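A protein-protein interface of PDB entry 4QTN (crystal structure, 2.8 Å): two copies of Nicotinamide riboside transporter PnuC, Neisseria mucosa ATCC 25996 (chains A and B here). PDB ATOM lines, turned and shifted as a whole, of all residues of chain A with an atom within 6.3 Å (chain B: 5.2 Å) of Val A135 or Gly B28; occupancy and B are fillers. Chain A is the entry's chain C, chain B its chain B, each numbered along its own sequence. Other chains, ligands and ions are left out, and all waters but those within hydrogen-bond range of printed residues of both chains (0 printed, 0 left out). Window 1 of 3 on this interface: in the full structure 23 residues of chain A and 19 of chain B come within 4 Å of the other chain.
Hydrophobic or aromatic side chains of chain B that line the printed part of chain A: Leu B24, Met B25, Ala B31 and Val B32.
Among the printed residues, no Asp or Glu carboxylate lies within 4 Å of a Lys or Arg side-chain nitrogen of the other chain.
Among the printed residues, pairs that only touch across the chains: Trp A131 with Met B25 (3.7 Å), Leu A132 with Leu B24 (3.8 Å), Val A135 with Gly B28 (3.7 Å), Val A139 with Ala B31 (3.998 Å) and Val A139 with Val B32 (3.8 Å).
Of chain B, only Gly B28 (3.7 Å) comes within 4 Å of Val A135.
Printed residues of chain B within 4 Å of Trp A131: Met B25.
Of the printed residues of chain A, Leu B24 touches Leu A132.
Of the printed residues of chain A, Met B25 touches Trp A131 (3.7 Å).
Of the printed residues of chain B, Val A139 touches Ala B31 and Val B32.
Of the printed residues of chain B, Leu A132 touches Leu B24 (3.8 Å).
Ile B29 touches none of the printed residues of chain A.
Leu B27 touches none of the printed residues of chain A.
The nearest residue of chain B that does not touch Val A135 is Met B25 (4.2 Å).
The nearest residue of chain A that does not touch Gly B28 is Val A139 (4.1 Å).
No position is printed for both chains.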
ATOM      1  N   GLN A 130     -27.081   5.977  26.567  1.00  0.00           N
ATOM      2  CA  GLN A 130     -28.222   5.869  25.656  1.00  0.00           C
ATOM      3  C   GLN A 130     -27.880   6.314  24.227  1.00  0.00           C
ATOM      4  O   GLN A 130     -28.304   5.684  23.260  1.00  0.00           O
ATOM      5  CB  GLN A 130     -29.386   6.697  26.175  1.00  0.00           C
ATOM      6  CG  GLN A 130     -29.752   6.448  27.617  1.00  0.00           C
ATOM      7  CD  GLN A 130     -31.104   7.032  27.957  1.00  0.00           C
ATOM      8  OE1 GLN A 130     -31.296   8.247  27.920  1.00  0.00           O
ATOM      9  NE2 GLN A 130     -32.061   6.166  28.275  1.00  0.00           N
ATOM     10  N   TRP A 131     -27.134   7.418  24.116  1.00  0.00           N
ATOM     11  CA  TRP A 131     -26.657   7.950  22.835  1.00  0.00           C
ATOM     12  C   TRP A 131     -25.702   6.974  22.151  1.00  0.00           C
ATOM     13  O   TRP A 131     -25.967   6.527  21.021  1.00  0.00           O
ATOM     14  CB  TRP A 131     -25.953   9.306  23.076  1.00  0.00           C
ATOM     15  CG  TRP A 131     -25.517  10.128  21.800  1.00  0.00           C
ATOM     16  CD1 TRP A 131     -24.277  10.670  21.556  1.00  0.00           C
ATOM     17  CD2 TRP A 131     -26.347  10.538  20.701  1.00  0.00           C
ATOM     18  NE1 TRP A 131     -24.285  11.355  20.371  1.00  0.00           N
ATOM     19  CE2 TRP A 131     -25.540  11.290  19.827  1.00  0.00           C
ATOM     20  CE3 TRP A 131     -27.688  10.322  20.362  1.00  0.00           C
ATOM     21  CZ2 TRP A 131     -26.027  11.828  18.649  1.00  0.00           C
ATOM     22  CZ3 TRP A 131     -28.174  10.876  19.179  1.00  0.00           C
ATOM     23  CH2 TRP A 131     -27.350  11.614  18.347  1.00  0.00           C
ATOM     24  N   LEU A 132     -24.598   6.629  22.841  1.00  0.00           N
ATOM     25  CA  LEU A 132     -23.551   5.775  22.253  1.00  0.00           C
ATOM     26  C   LEU A 132     -24.145   4.532  21.576  1.00  0.00           C
ATOM     27  O   LEU A 132     -23.643   4.079  20.556  1.00  0.00           O
ATOM     28  CB  LEU A 132     -22.498   5.374  23.296  1.00  0.00           C
ATOM     29  CG  LEU A 132     -21.475   4.319  22.823  1.00  0.00           C
ATOM     30  CD1 LEU A 132     -20.396   4.935  21.938  1.00  0.00           C
ATOM     31  CD2 LEU A 132     -20.861   3.563  23.989  1.00  0.00           C
ATOM     32  N   LEU A 133     -25.221   4.006  22.148  1.00  0.00           N
ATOM     33  CA  LEU A 133     -25.999   2.977  21.494  1.00  0.00           C
ATOM     34  C   LEU A 133     -26.525   3.430  20.142  1.00  0.00           C
ATOM     35  O   LEU A 133     -26.255   2.792  19.130  1.00  0.00           O
ATOM     36  CB  LEU A 133     -27.165   2.589  22.356  1.00  0.00           C
ATOM     37  CG  LEU A 133     -27.029   1.281  23.075  1.00  0.00           C
ATOM     38  CD1 LEU A 133     -25.848   1.364  24.026  1.00  0.00           C
ATOM     39  CD2 LEU A 133     -28.335   0.975  23.805  1.00  0.00           C
ATOM     40  N   VAL A 134     -27.302   4.521  20.132  1.00  0.00           N
ATOM     41  CA  VAL A 134     -27.972   4.992  18.903  1.00  0.00           C
ATOM     42  C   VAL A 134     -26.977   5.246  17.759  1.00  0.00           C
ATOM     43  O   VAL A 134     -27.232   4.853  16.633  1.00  0.00           O
ATOM     44  CB  VAL A 134     -28.844   6.259  19.148  1.00  0.00           C
ATOM     45  CG1 VAL A 134     -29.472   6.731  17.851  1.00  0.00           C
ATOM     46  CG2 VAL A 134     -29.936   5.977  20.160  1.00  0.00           C
ATOM     47  N   VAL A 135     -25.847   5.893  18.065  1.00  0.00           N
ATOM     48  CA  VAL A 135     -24.760   6.097  17.087  1.00  0.00           C
ATOM     49  C   VAL A 135     -24.314   4.775  16.458  1.00  0.00           C
ATOM     50  O   VAL A 135     -24.157   4.677  15.238  1.00  0.00           O
ATOM     51  CB  VAL A 135     -23.530   6.787  17.746  1.00  0.00           C
ATOM     52  CG1 VAL A 135     -22.239   6.489  16.976  1.00  0.00           C
ATOM     53  CG2 VAL A 135     -23.758   8.287  17.880  1.00  0.00           C
ATOM     54  N   ALA A 136     -24.091   3.770  17.310  1.00  0.00           N
ATOM     55  CA  ALA A 136     -23.749   2.418  16.883  1.00  0.00           C
ATOM     56  C   ALA A 136     -24.841   1.812  16.015  1.00  0.00           C
ATOM     57  O   ALA A 136     -24.583   1.368  14.905  1.00  0.00           O
ATOM     58  CB  ALA A 136     -23.510   1.547  18.093  1.00  0.00           C
ATOM     59  N   ALA A 137     -26.059   1.780  16.545  1.00  0.00           N
ATOM     60  CA  ALA A 137     -27.246   1.427  15.777  1.00  0.00           C
ATOM     61  C   ALA A 137     -27.164   1.869  14.303  1.00  0.00           C
ATOM     62  O   ALA A 137     -27.416   1.065  13.397  1.00  0.00           O
ATOM     63  CB  ALA A 137     -28.492   2.002  16.440  1.00  0.00           C
ATOM     64  N   SER A 138     -26.801   3.137  14.068  1.00  0.00           N
ATOM     65  CA  SER A 138     -26.744   3.685  12.700  1.00  0.00           C
ATOM     66  C   SER A 138     -25.633   3.068  11.872  1.00  0.00           C
ATOM     67  O   SER A 138     -25.780   2.901  10.671  1.00  0.00           O
ATOM     68  CB  SER A 138     -26.578   5.187  12.726  1.00  0.00           C
ATOM     69  OG  SER A 138     -27.370   5.740  13.733  1.00  0.00           O
ATOM     70  N   VAL A 139     -24.521   2.738  12.517  1.00  0.00           N
ATOM     71  CA  VAL A 139     -23.394   2.144  11.831  1.00  0.00           C
ATOM     72  C   VAL A 139     -23.699   0.671  11.484  1.00  0.00           C
ATOM     73  O   VAL A 139     -23.354   0.187  10.398  1.00  0.00           O
ATOM     74  CB  VAL A 139     -22.117   2.285  12.681  1.00  0.00           C
ATOM     75  CG1 VAL A 139     -20.921   1.634  12.009  1.00  0.00           C
ATOM     76  CG2 VAL A 139     -21.840   3.749  12.941  1.00  0.00           C
ATOM     77  N   VAL A 140     -24.356  -0.025  12.409  1.00  0.00           N
ATOM     78  CA  VAL A 140     -24.936  -1.344  12.148  1.00  0.00           C
ATOM     79  C   VAL A 140     -25.878  -1.297  10.928  1.00  0.00           C
ATOM     80  O   VAL A 140     -25.658  -1.996   9.923  1.00  0.00           O
ATOM     81  CB  VAL A 140     -25.725  -1.842  13.382  1.00  0.00           C
ATOM     82  CG1 VAL A 140     -26.616  -3.027  13.020  1.00  0.00           C
ATOM     83  CG2 VAL A 140     -24.775  -2.195  14.515  1.00  0.00           C
ATOM     84  N   LEU B  24     -19.068  12.089  20.032  1.00  0.00           N
ATOM     85  CA  LEU B  24     -19.508  10.767  19.595  1.00  0.00           C
ATOM     86  C   LEU B  24     -20.182  10.823  18.233  1.00  0.00           C
ATOM     87  O   LEU B  24     -19.847  10.062  17.347  1.00  0.00           O
ATOM     88  CB  LEU B  24     -20.422  10.097  20.623  1.00  0.00           C
ATOM     89  CG  LEU B  24     -19.860   9.618  21.980  1.00  0.00           C
ATOM     90  CD1 LEU B  24     -20.929   8.817  22.729  1.00  0.00           C
ATOM     91  CD2 LEU B  24     -18.563   8.812  21.853  1.00  0.00           C
ATOM     92  N   MET B  25     -21.125  11.743  18.070  1.00  0.00           N
ATOM     93  CA  MET B  25     -21.838  11.896  16.790  1.00  0.00           C
ATOM     94  C   MET B  25     -20.872  12.202  15.666  1.00  0.00           C
ATOM     95  O   MET B  25     -21.120  11.846  14.517  1.00  0.00           O
ATOM     96  CB  MET B  25     -22.928  12.966  16.925  1.00  0.00           C
ATOM     97  CG  MET B  25     -22.783  14.151  15.965  1.00  0.00           C
ATOM     98  SD  MET B  25     -24.528  14.484  15.122  1.00  0.00           S
ATOM     99  CE  MET B  25     -24.848  12.619  14.597  1.00  0.00           C
ATOM    100  N   PHE B  26     -19.751  12.845  15.992  1.00  0.00           N
ATOM    101  CA  PHE B  26     -18.749  13.155  14.984  1.00  0.00           C
ATOM    102  C   PHE B  26     -18.069  11.914  14.512  1.00  0.00           C
ATOM    103  O   PHE B  26     -17.826  11.767  13.330  1.00  0.00           O
ATOM    104  CB  PHE B  26     -17.705  14.127  15.513  1.00  0.00           C
ATOM    105  CG  PHE B  26     -18.111  15.554  15.408  1.00  0.00           C
ATOM    106  CD1 PHE B  26     -19.131  15.944  14.518  1.00  0.00           C
ATOM    107  CD2 PHE B  26     -17.480  16.524  16.175  1.00  0.00           C
ATOM    108  CE1 PHE B  26     -19.508  17.263  14.409  1.00  0.00           C
ATOM    109  CE2 PHE B  26     -17.845  17.850  16.060  1.00  0.00           C
ATOM    110  CZ  PHE B  26     -18.864  18.220  15.176  1.00  0.00           C
ATOM    111  N   LEU B  27     -17.754  11.021  15.455  1.00  0.00           N
ATOM    112  CA  LEU B  27     -17.047   9.785  15.157  1.00  0.00           C
ATOM    113  C   LEU B  27     -17.946   8.799  14.448  1.00  0.00           C
ATOM    114  O   LEU B  27     -17.543   8.159  13.490  1.00  0.00           O
ATOM    115  CB  LEU B  27     -16.477   9.183  16.433  1.00  0.00           C
ATOM    116  CG  LEU B  27     -15.336  10.019  17.044  1.00  0.00           C
ATOM    117  CD1 LEU B  27     -14.804   9.431  18.353  1.00  0.00           C
ATOM    118  CD2 LEU B  27     -14.212  10.230  16.033  1.00  0.00           C
ATOM    119  N   GLY B  28     -19.180   8.706  14.905  1.00  0.00           N
ATOM    120  CA  GLY B  28     -20.212   7.958  14.193  1.00  0.00           C
ATOM    121  C   GLY B  28     -20.355   8.323  12.722  1.00  0.00           C
ATOM    122  O   GLY B  28     -20.376   7.440  11.871  1.00  0.00           O
ATOM    123  N   ILE B  29     -20.446   9.626  12.414  1.00  0.00           N
ATOM    124  CA  ILE B  29     -20.562  10.079  10.998  1.00  0.00           C
ATOM    125  C   ILE B  29     -19.322   9.737  10.191  1.00  0.00           C
ATOM    126  O   ILE B  29     -19.414   9.435   9.007  1.00  0.00           O
ATOM    127  CB  ILE B  29     -20.847  11.594  10.869  1.00  0.00           C
ATOM    128  CG1 ILE B  29     -22.175  11.941  11.524  1.00  0.00           C
ATOM    129  CG2 ILE B  29     -20.887  12.012   9.406  1.00  0.00           C
ATOM    130  CD1 ILE B  29     -23.266  10.912  11.293  1.00  0.00           C
ATOM    131  N   GLN B  30     -18.166   9.795  10.842  1.00  0.00           N
ATOM    132  CA  GLN B  30     -16.918   9.359  10.248  1.00  0.00           C
ATOM    133  C   GLN B  30     -16.976   7.832   9.940  1.00  0.00           C
ATOM    134  O   GLN B  30     -16.497   7.377   8.882  1.00  0.00           O
ATOM    135  CB  GLN B  30     -15.749   9.701  11.197  1.00  0.00           C
ATOM    136  CG  GLN B  30     -14.479  10.233  10.530  1.00  0.00           C
ATOM    137  CD  GLN B  30     -14.744  11.129   9.333  1.00  0.00           C
ATOM    138  OE1 GLN B  30     -14.582  10.712   8.186  1.00  0.00           O
ATOM    139  NE2 GLN B  30     -15.117  12.365   9.589  1.00  0.00           N
ATOM    140  N   ALA B  31     -17.605   7.073  10.844  1.00  0.00           N
ATOM    141  CA  ALA B  31     -17.730   5.625  10.712  1.00  0.00           C
ATOM    142  C   ALA B  31     -18.691   5.236   9.613  1.00  0.00           C
ATOM    143  O   ALA B  31     -18.329   4.501   8.710  1.00  0.00           O
ATOM    144  CB  ALA B  31     -18.161   5.014  12.021  1.00  0.00           C
ATOM    145  N   VAL B  32     -19.926   5.709   9.701  1.00  0.00           N
ATOM    146  CA  VAL B  32     -20.910   5.555   8.611  1.00  0.00           C
ATOM    147  C   VAL B  32     -20.325   5.843   7.203  1.00  0.00           C
ATOM    148  O   VAL B  32     -20.731   5.231   6.195  1.00  0.00           O
ATOM    149  CB  VAL B  32     -22.103   6.487   8.836  1.00  0.00           C
ATOM    150  CG1 VAL B  32     -23.188   6.260   7.776  1.00  0.00           C
ATOM    151  CG2 VAL B  32     -22.648   6.311  10.240  1.00  0.00           C
ATOM    152  N   VAL B  33     -19.394   6.793   7.147  1.00  0.00           N
ATOM    153  CA  VAL B  33     -18.700   7.142   5.909  1.00  0.00           C
ATOM    154  C   VAL B  33     -17.812   6.005   5.432  1.00  0.00           C
ATOM    155  O   VAL B  33     -17.708   5.759   4.241  1.00  0.00           O
ATOM    156  CB  VAL B  33     -17.886   8.454   6.079  1.00  0.00           C
ATOM    157  CG1 VAL B  33     -16.384   8.237   5.864  1.00  0.00           C
ATOM    158  CG2 VAL B  33     -18.451   9.546   5.183  1.00  0.00           C
